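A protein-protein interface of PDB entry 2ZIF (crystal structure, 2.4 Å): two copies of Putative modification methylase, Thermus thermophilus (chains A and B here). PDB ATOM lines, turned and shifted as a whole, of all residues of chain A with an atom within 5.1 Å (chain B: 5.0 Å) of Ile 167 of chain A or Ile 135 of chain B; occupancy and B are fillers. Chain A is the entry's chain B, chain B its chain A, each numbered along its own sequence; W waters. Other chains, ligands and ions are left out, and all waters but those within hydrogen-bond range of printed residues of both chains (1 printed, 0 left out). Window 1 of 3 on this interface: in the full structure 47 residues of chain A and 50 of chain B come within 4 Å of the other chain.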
ATOM      1  N   GLY A  98       4.809  21.886   7.531  1.00  0.00           N
ATOM      2  CA  GLY A  98       4.275  21.243   6.354  1.00  0.00           C
ATOM      3  C   GLY A  98       4.917  19.877   6.353  1.00  0.00           C
ATOM      4  O   GLY A  98       6.087  19.757   6.720  1.00  0.00           O
ATOM      5  N   ILE A 135      -5.816  24.752   9.336  1.00  0.00           N
ATOM      6  CA  ILE A 135      -5.207  24.346   8.082  1.00  0.00           C
ATOM      7  C   ILE A 135      -4.871  25.571   7.252  1.00  0.00           C
ATOM      8  O   ILE A 135      -5.743  26.345   6.902  1.00  0.00           O
ATOM      9  CB  ILE A 135      -6.139  23.472   7.227  1.00  0.00           C
ATOM     10  CG1 ILE A 135      -6.535  22.213   7.996  1.00  0.00           C
ATOM     11  CG2 ILE A 135      -5.444  23.141   5.891  1.00  0.00           C
ATOM     12  CD1 ILE A 135      -5.363  21.468   8.653  1.00  0.00           C
ATOM     13  N   TRP A 136      -3.601  25.759   6.956  1.00  0.00           N
ATOM     14  CA  TRP A 136      -3.212  26.871   6.124  1.00  0.00           C
ATOM     15  C   TRP A 136      -3.195  26.357   4.688  1.00  0.00           C
ATOM     16  O   TRP A 136      -2.315  25.584   4.296  1.00  0.00           O
ATOM     17  CB  TRP A 136      -1.831  27.377   6.512  1.00  0.00           C
ATOM     18  CG  TRP A 136      -1.321  28.440   5.594  1.00  0.00           C
ATOM     19  CD1 TRP A 136      -2.063  29.339   4.882  1.00  0.00           C
ATOM     20  CD2 TRP A 136       0.050  28.767   5.346  1.00  0.00           C
ATOM     21  NE1 TRP A 136      -1.239  30.207   4.210  1.00  0.00           N
ATOM     22  CE2 TRP A 136       0.064  29.880   4.480  1.00  0.00           C
ATOM     23  CE3 TRP A 136       1.267  28.230   5.776  1.00  0.00           C
ATOM     24  CZ2 TRP A 136       1.251  30.470   4.035  1.00  0.00           C
ATOM     25  CZ3 TRP A 136       2.448  28.818   5.335  1.00  0.00           C
ATOM     26  CH2 TRP A 136       2.428  29.927   4.473  1.00  0.00           C
ATOM     27  N   HIS A 137      -4.203  26.749   3.921  1.00  0.00           N
ATOM     28  CA  HIS A 137      -4.268  26.352   2.531  1.00  0.00           C
ATOM     29  C   HIS A 137      -3.306  27.309   1.837  1.00  0.00           C
ATOM     30  O   HIS A 137      -3.691  28.353   1.337  1.00  0.00           O
ATOM     31  CB  HIS A 137      -5.687  26.519   1.993  1.00  0.00           C
ATOM     32  CG  HIS A 137      -5.937  25.752   0.737  1.00  0.00           C
ATOM     33  ND1 HIS A 137      -7.181  25.658   0.154  1.00  0.00           N
ATOM     34  CD2 HIS A 137      -5.095  25.048  -0.056  1.00  0.00           C
ATOM     35  CE1 HIS A 137      -7.096  24.932  -0.945  1.00  0.00           C
ATOM     36  NE2 HIS A 137      -5.841  24.550  -1.095  1.00  0.00           N
ATOM     37  N   LYS A 138      -2.040  26.932   1.861  1.00  0.00           N
ATOM     38  CA  LYS A 138      -0.959  27.715   1.299  1.00  0.00           C
ATOM     39  C   LYS A 138      -1.064  27.894  -0.210  1.00  0.00           C
ATOM     40  O   LYS A 138      -1.095  29.018  -0.703  1.00  0.00           O
ATOM     41  CB  LYS A 138       0.367  27.044   1.665  1.00  0.00           C
ATOM     42  CG  LYS A 138       1.588  27.923   1.497  1.00  0.00           C
ATOM     43  CD  LYS A 138       2.834  27.273   2.107  1.00  0.00           C
ATOM     44  CE  LYS A 138       4.079  28.074   1.749  1.00  0.00           C
ATOM     45  NZ  LYS A 138       5.333  27.539   2.342  1.00  0.00           N
ATOM     46  N   THR A 165       1.098  18.654  -2.521  1.00  0.00           N
ATOM     47  CA  THR A 165       0.918  19.389  -1.284  1.00  0.00           C
ATOM     48  C   THR A 165       0.358  20.803  -1.464  1.00  0.00           C
ATOM     49  O   THR A 165       0.933  21.643  -2.159  1.00  0.00           O
ATOM     50  CB  THR A 165       2.239  19.499  -0.516  1.00  0.00           C
ATOM     51  OG1 THR A 165       2.779  18.193  -0.322  1.00  0.00           O
ATOM     52  CG2 THR A 165       2.012  20.150   0.840  1.00  0.00           C
ATOM     53  N   GLU A 166      -0.764  21.067  -0.815  1.00  0.00           N
ATOM     54  CA  GLU A 166      -1.369  22.382  -0.891  1.00  0.00           C
ATOM     55  C   GLU A 166      -1.401  23.025   0.485  1.00  0.00           C
ATOM     56  O   GLU A 166      -1.514  24.241   0.613  1.00  0.00           O
ATOM     57  CB  GLU A 166      -2.801  22.277  -1.402  1.00  0.00           C
ATOM     58  CG  GLU A 166      -2.928  21.727  -2.801  1.00  0.00           C
ATOM     59  CD  GLU A 166      -4.367  21.632  -3.237  1.00  0.00           C
ATOM     60  OE1 GLU A 166      -5.100  22.623  -3.051  1.00  0.00           O
ATOM     61  OE2 GLU A 166      -4.770  20.579  -3.770  1.00  0.00           O
ATOM     62  N   ILE A 167      -1.276  22.208   1.518  1.00  0.00           N
ATOM     63  CA  ILE A 167      -1.390  22.728   2.870  1.00  0.00           C
ATOM     64  C   ILE A 167      -0.212  22.585   3.818  1.00  0.00           C
ATOM     65  O   ILE A 167       0.730  21.823   3.591  1.00  0.00           O
ATOM     66  CB  ILE A 167      -2.595  22.083   3.566  1.00  0.00           C
ATOM     67  CG1 ILE A 167      -2.274  20.612   3.864  1.00  0.00           C
ATOM     68  CG2 ILE A 167      -3.836  22.187   2.672  1.00  0.00           C
ATOM     69  CD1 ILE A 167      -3.394  19.829   4.514  1.00  0.00           C
ATOM     70  N   GLU A 168      -0.304  23.353   4.895  1.00  0.00           N
ATOM     71  CA  GLU A 168       0.654  23.318   5.978  1.00  0.00           C
ATOM     72  C   GLU A 168      -0.229  23.273   7.206  1.00  0.00           C
ATOM     73  O   GLU A 168      -1.405  23.636   7.145  1.00  0.00           O
ATOM     74  CB  GLU A 168       1.554  24.547   5.987  1.00  0.00           C
ATOM     75  CG  GLU A 168       2.770  24.362   5.104  1.00  0.00           C
ATOM     76  CD  GLU A 168       3.923  25.209   5.549  1.00  0.00           C
ATOM     77  OE1 GLU A 168       4.163  25.263   6.775  1.00  0.00           O
ATOM     78  OE2 GLU A 168       4.595  25.809   4.684  1.00  0.00           O
ATOM     79  N   TYR A 169       0.322  22.808   8.318  1.00  0.00           N
ATOM     80  CA  TYR A 169      -0.455  22.668   9.535  1.00  0.00           C
ATOM     81  C   TYR A 169      -0.100  23.683  10.599  1.00  0.00           C
ATOM     82  O   TYR A 169       1.071  23.984  10.822  1.00  0.00           O
ATOM     83  CB  TYR A 169      -0.247  21.270  10.098  1.00  0.00           C
ATOM     84  CG  TYR A 169      -0.607  20.168   9.137  1.00  0.00           C
ATOM     85  CD1 TYR A 169      -1.883  19.602   9.136  1.00  0.00           C
ATOM     86  CD2 TYR A 169       0.328  19.695   8.219  1.00  0.00           C
ATOM     87  CE1 TYR A 169      -2.218  18.585   8.241  1.00  0.00           C
ATOM     88  CE2 TYR A 169       0.008  18.687   7.322  1.00  0.00           C
ATOM     89  CZ  TYR A 169      -1.267  18.134   7.338  1.00  0.00           C
ATOM     90  OH  TYR A 169      -1.575  17.132   6.446  1.00  0.00           O
ATOM     91  N   ILE A 204      -9.883  26.732   8.533  1.00  0.00           N
ATOM     92  CA  ILE A 204      -9.076  26.803   7.314  1.00  0.00           C
ATOM     93  C   ILE A 204      -8.803  28.241   6.871  1.00  0.00           C
ATOM     94  O   ILE A 204      -9.714  29.069   6.799  1.00  0.00           O
ATOM     95  CB  ILE A 204      -9.747  26.036   6.146  1.00  0.00           C
ATOM     96  CG1 ILE A 204      -9.972  24.572   6.557  1.00  0.00           C
ATOM     97  CG2 ILE A 204      -8.874  26.122   4.906  1.00  0.00           C
ATOM     98  CD1 ILE A 204     -10.569  23.702   5.491  1.00  0.00           C
ATOM     99  N   PRO B 133      -2.622  13.424   3.215  1.00  0.00           N
ATOM    100  CA  PRO B 133      -4.044  13.115   3.343  1.00  0.00           C
ATOM    101  C   PRO B 133      -4.857  14.199   2.657  1.00  0.00           C
ATOM    102  O   PRO B 133      -4.346  15.277   2.341  1.00  0.00           O
ATOM    103  CB  PRO B 133      -4.255  13.104   4.849  1.00  0.00           C
ATOM    104  CG  PRO B 133      -3.356  14.220   5.294  1.00  0.00           C
ATOM    105  CD  PRO B 133      -2.098  14.046   4.445  1.00  0.00           C
ATOM    106  N   ILE B 134      -6.116  13.901   2.403  1.00  0.00           N
ATOM    107  CA  ILE B 134      -6.984  14.879   1.806  1.00  0.00           C
ATOM    108  C   ILE B 134      -7.817  15.389   2.987  1.00  0.00           C
ATOM    109  O   ILE B 134      -8.259  14.599   3.826  1.00  0.00           O
ATOM    110  CB  ILE B 134      -7.896  14.236   0.718  1.00  0.00           C
ATOM    111  CG1 ILE B 134      -7.048  13.755  -0.469  1.00  0.00           C
ATOM    112  CG2 ILE B 134      -8.934  15.249   0.240  1.00  0.00           C
ATOM    113  CD1 ILE B 134      -7.823  12.951  -1.506  1.00  0.00           C
ATOM    114  N   ILE B 135      -8.001  16.703   3.065  1.00  0.00           N
ATOM    115  CA  ILE B 135      -8.784  17.309   4.133  1.00  0.00           C
ATOM    116  C   ILE B 135     -10.249  17.390   3.733  1.00  0.00           C
ATOM    117  O   ILE B 135     -10.595  18.064   2.750  1.00  0.00           O
ATOM    118  CB  ILE B 135      -8.312  18.743   4.438  1.00  0.00           C
ATOM    119  CG1 ILE B 135      -6.841  18.736   4.865  1.00  0.00           C
ATOM    120  CG2 ILE B 135      -9.213  19.371   5.512  1.00  0.00           C
ATOM    121  CD1 ILE B 135      -6.562  17.869   6.085  1.00  0.00           C
ATOM    122  N   TRP B 136     -11.113  16.692   4.463  1.00  0.00           N
ATOM    123  CA  TRP B 136     -12.530  16.774   4.148  1.00  0.00           C
ATOM    124  C   TRP B 136     -13.146  17.923   4.951  1.00  0.00           C
ATOM    125  O   TRP B 136     -13.291  17.850   6.178  1.00  0.00           O
ATOM    126  CB  TRP B 136     -13.259  15.466   4.468  1.00  0.00           C
ATOM    127  CG  TRP B 136     -14.739  15.551   4.214  1.00  0.00           C
ATOM    128  CD1 TRP B 136     -15.379  16.363   3.309  1.00  0.00           C
ATOM    129  CD2 TRP B 136     -15.763  14.768   4.839  1.00  0.00           C
ATOM    130  NE1 TRP B 136     -16.731  16.128   3.335  1.00  0.00           N
ATOM    131  CE2 TRP B 136     -16.998  15.158   4.263  1.00  0.00           C
ATOM    132  CE3 TRP B 136     -15.759  13.773   5.824  1.00  0.00           C
ATOM    133  CZ2 TRP B 136     -18.218  14.587   4.644  1.00  0.00           C
ATOM    134  CZ3 TRP B 136     -16.974  13.200   6.204  1.00  0.00           C
ATOM    135  CH2 TRP B 136     -18.186  13.611   5.613  1.00  0.00           C
ATOM    136  N   HIS B 137     -13.483  18.995   4.248  1.00  0.00           N
ATOM    137  CA  HIS B 137     -14.084  20.143   4.884  1.00  0.00           C
ATOM    138  C   HIS B 137     -15.594  19.928   4.978  1.00  0.00           C
ATOM    139  O   HIS B 137     -16.346  20.451   4.169  1.00  0.00           O
ATOM    140  CB  HIS B 137     -13.778  21.403   4.085  1.00  0.00           C
ATOM    141  CG  HIS B 137     -13.990  22.665   4.859  1.00  0.00           C
ATOM    142  ND1 HIS B 137     -13.723  23.912   4.340  1.00  0.00           N
ATOM    143  CD2 HIS B 137     -14.443  22.869   6.118  1.00  0.00           C
ATOM    144  CE1 HIS B 137     -14.005  24.832   5.244  1.00  0.00           C
ATOM    145  NE2 HIS B 137     -14.443  24.224   6.333  1.00  0.00           N
ATOM    146  N   ILE B 167     -13.518  19.976   9.943  1.00  0.00           N
ATOM    147  CA  ILE B 167     -12.933  18.998   9.058  1.00  0.00           C
ATOM    148  C   ILE B 167     -12.748  17.602   9.611  1.00  0.00           C
ATOM    149  O   ILE B 167     -12.719  17.386  10.815  1.00  0.00           O
ATOM    150  CB  ILE B 167     -11.514  19.443   8.629  1.00  0.00           C
ATOM    151  CG1 ILE B 167     -10.578  19.295   9.835  1.00  0.00           C
ATOM    152  CG2 ILE B 167     -11.520  20.889   8.119  1.00  0.00           C
ATOM    153  CD1 ILE B 167      -9.124  19.412   9.526  1.00  0.00           C
ATOM    154  N   GLU B 168     -12.606  16.665   8.687  1.00  0.00           N
ATOM    155  CA  GLU B 168     -12.279  15.296   9.025  1.00  0.00           C
ATOM    156  C   GLU B 168     -11.070  15.041   8.138  1.00  0.00           C
ATOM    157  O   GLU B 168     -10.860  15.747   7.144  1.00  0.00           O
ATOM    158  CB  GLU B 168     -13.425  14.333   8.723  1.00  0.00           C
ATOM    159  CG  GLU B 168     -14.391  14.230   9.896  1.00  0.00           C
ATOM    160  CD  GLU B 168     -15.343  13.068   9.782  1.00  0.00           C
ATOM    161  OE1 GLU B 168     -14.886  11.963   9.420  1.00  0.00           O
ATOM    162  OE2 GLU B 168     -16.543  13.253  10.067  1.00  0.00           O
ATOM    163  N   TYR B 169     -10.256  14.065   8.505  1.00  0.00           N
ATOM    164  CA  TYR B 169      -9.064  13.764   7.737  1.00  0.00           C
ATOM    165  C   TYR B 169      -9.238  12.487   6.945  1.00  0.00           C
ATOM    166  O   TYR B 169      -9.827  11.508   7.431  1.00  0.00           O
ATOM    167  CB  TYR B 169      -7.859  13.600   8.668  1.00  0.00           C
ATOM    168  CG  TYR B 169      -7.567  14.791   9.551  1.00  0.00           C
ATOM    169  CD1 TYR B 169      -8.299  15.025  10.719  1.00  0.00           C
ATOM    170  CD2 TYR B 169      -6.554  15.681   9.228  1.00  0.00           C
ATOM    171  CE1 TYR B 169      -8.021  16.119  11.544  1.00  0.00           C
ATOM    172  CE2 TYR B 169      -6.267  16.783  10.044  1.00  0.00           C
ATOM    173  CZ  TYR B 169      -7.002  16.993  11.197  1.00  0.00           C
ATOM    174  OH  TYR B 169      -6.710  18.076  11.997  1.00  0.00           O
ATOM    175  N   GLN B 203      -5.977  18.452  -2.435  1.00  0.00           N
ATOM    176  CA  GLN B 203      -5.841  18.204  -1.018  1.00  0.00           C
ATOM    177  C   GLN B 203      -7.046  18.573  -0.140  1.00  0.00           C
ATOM    178  O   GLN B 203      -7.176  18.072   0.978  1.00  0.00           O
ATOM    179  CB  GLN B 203      -4.548  18.854  -0.505  1.00  0.00           C
ATOM    180  CG  GLN B 203      -4.176  18.372   0.890  1.00  0.00           C
ATOM    181  CD  GLN B 203      -2.696  18.457   1.193  1.00  0.00           C
ATOM    182  OE1 GLN B 203      -2.005  19.384   0.756  1.00  0.00           O
ATOM    183  NE2 GLN B 203      -2.203  17.496   1.968  1.00  0.00           N
ATOM    184  N   ILE B 204      -7.936  19.425  -0.639  1.00  0.00           N
ATOM    185  CA  ILE B 204      -9.108  19.792   0.147  1.00  0.00           C
ATOM    186  C   ILE B 204     -10.420  19.631  -0.615  1.00  0.00           C
ATOM    187  O   ILE B 204     -10.577  20.147  -1.720  1.00  0.00           O
ATOM    188  CB  ILE B 204      -9.015  21.256   0.671  1.00  0.00           C
ATOM    189  CG1 ILE B 204      -7.780  21.425   1.562  1.00  0.00           C
ATOM    190  CG2 ILE B 204     -10.259  21.588   1.496  1.00  0.00           C
ATOM    191  CD1 ILE B 204      -7.513  22.855   2.003  1.00  0.00           C
ATOM    192  N   TRP B 205     -11.353  18.888  -0.029  1.00  0.00           N
ATOM    193  CA  TRP B 205     -12.663  18.700  -0.626  1.00  0.00           C
ATOM    194  C   TRP B 205     -13.656  19.523   0.172  1.00  0.00           C
ATOM    195  O   TRP B 205     -13.871  19.268   1.355  1.00  0.00           O
ATOM    196  CB  TRP B 205     -13.101  17.243  -0.588  1.00  0.00           C
ATOM    197  CG  TRP B 205     -12.342  16.339  -1.506  1.00  0.00           C
ATOM    198  CD1 TRP B 205     -11.481  16.704  -2.500  1.00  0.00           C
ATOM    199  CD2 TRP B 205     -12.379  14.910  -1.508  1.00  0.00           C
ATOM    200  NE1 TRP B 205     -10.974  15.591  -3.117  1.00  0.00           N
ATOM    201  CE2 TRP B 205     -11.508  14.472  -2.531  1.00  0.00           C
ATOM    202  CE3 TRP B 205     -13.067  13.953  -0.743  1.00  0.00           C
ATOM    203  CZ2 TRP B 205     -11.300  13.117  -2.813  1.00  0.00           C
ATOM    204  CZ3 TRP B 205     -12.863  12.607  -1.022  1.00  0.00           C
ATOM    205  CH2 TRP B 205     -11.981  12.203  -2.053  1.00  0.00           C
HETATM  206  O   HOH W   1      -0.213  17.490   3.816  1.00  0.00           O
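The side-chain amide oxygen (OE1) of Gln 203 of chain B sits at hydrogen-bond distance from the backbone NH (N) of Ile 167 of chain A.
The side-chain amide oxygen of Gln 203 of chain B is in hydrogen-bond range of the backbone NH of Glu 166 of chain A (2.6 Å).
NE2 of His 137 of chain A lies within hydrogen-bond range of OE1 of Glu 166 of chain A, at 2.8 Å.
The backbone NH (N) of Ile 135 of chain B sits at hydrogen-bond distance from the backbone carbonyl oxygen (O) of Gln 203 of chain B (2.6 Å).
The side-chain amide nitrogen of Gln 203 of chain B lies within hydrogen-bond range of the backbone carbonyl oxygen of Pro 133 of chain B, 3.1 Å away.
The backbone NH (N) of Lys 138 of chain A lies within hydrogen-bond range of the backbone carbonyl oxygen (O) of Glu 166 of chain A, 3.0 Å away.
N of His 137 of chain B is in hydrogen-bond range of O of Trp 205 of chain B, at 2.9 Å.
The backbone carbonyl oxygen (O) of Ile 135 of chain B lies within hydrogen-bond range of the backbone NH (N) of Trp 205 of chain B.
Among the printed residues, pairs that only touch across the chains: Ile 204 of chain A with His 137 of chain B (3.4 Å), His 137 of chain A with Ile 204 of chain B (3.4 Å), Thr 165 of chain A with Gln 203 of chain B (3.5 Å), Tyr 169 of chain A with Pro 133 of chain B (3.6 Å), Ile 167 of chain A with Ile 135 of chain B (3.6 Å), Ile 167 of chain A with Ile 204 of chain B (3.8 Å) and Ile 204 of chain A with Ile 167 of chain B (3.97 Å).
Trp 136 of chain A touches none of the printed residues of chain B.
Printed residues of chain B within 4 Å of His 137 of chain A: Ile 204.
Printed residues of chain B within 4 Å of Thr 165 of chain A: Gln 203 (3.5 Å).
Of chain B, only Ile 135 (3.6 Å), Gln 203 (3.0 Å) and Ile 204 (3.8 Å) come within 4 Å of Ile 167 of chain A.
Printed residues of chain B within 4 Å of Tyr 169 of chain A: Pro 133 (3.6 Å).
Ile 135 of chain B touches just one residue of chain A: Ile 167.
Of the printed residues of chain A, Ile 204 of chain B touches His 137 (3.4 Å) and Ile 167 (3.8 Å).
Of the 11 printed residues of chain B, 6 touch a printed residue of chain A.
Printed residues of chain B that touch a printed residue of chain A: Pro 133, Ile 135, His 137, Ile 167, Gln 203 and Ile 204.
Hydrophobic or aromatic side chains of chain B within 4 Å of the printed part of chain A: Pro 133, Ile 135, His 137, Ile 167 and Ile 204.
Of the 11 printed residues of chain A, 6 touch a printed residue of chain B.
Hydrophobic or aromatic side chains of chain A within 4 Å of the printed part of chain B: His 137, Ile 167, Tyr 169 and Ile 204.
Among the printed residues, 9 pairs touch across the chains.
Among the printed residues, no Asp or Glu carboxylate lies within 4 Å of a Lys or Arg side-chain nitrogen of the other chain.
His 137 of chain A touches Ile 204 of chain B, and with the chains exchanged Ile 204 of chain A touches His 137 of chain B.
Ile 167 of chain A touches Ile 135 of chain B, but with the chains exchanged Ile 135 of chain A does not touch Ile 167 of chain B (4.1 Å).
Ile 167 of chain A touches Ile 204 of chain B, and with the chains exchanged Ile 204 of chain A touches Ile 167 of chain B.
Positions printed for both chains: 135, 136, 137, 167, 168, 169 and 204.
Of the 9 pairs that touch across the chains among the printed residues, 4 have their exchanged pair printed and touching as well.
Water W1 lies within hydrogen-bond range of the side-chain amide nitrogen (NE2) of Gln 203 of chain B and the side-chain hydroxyl (OH) of Tyr 169 of chain A.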
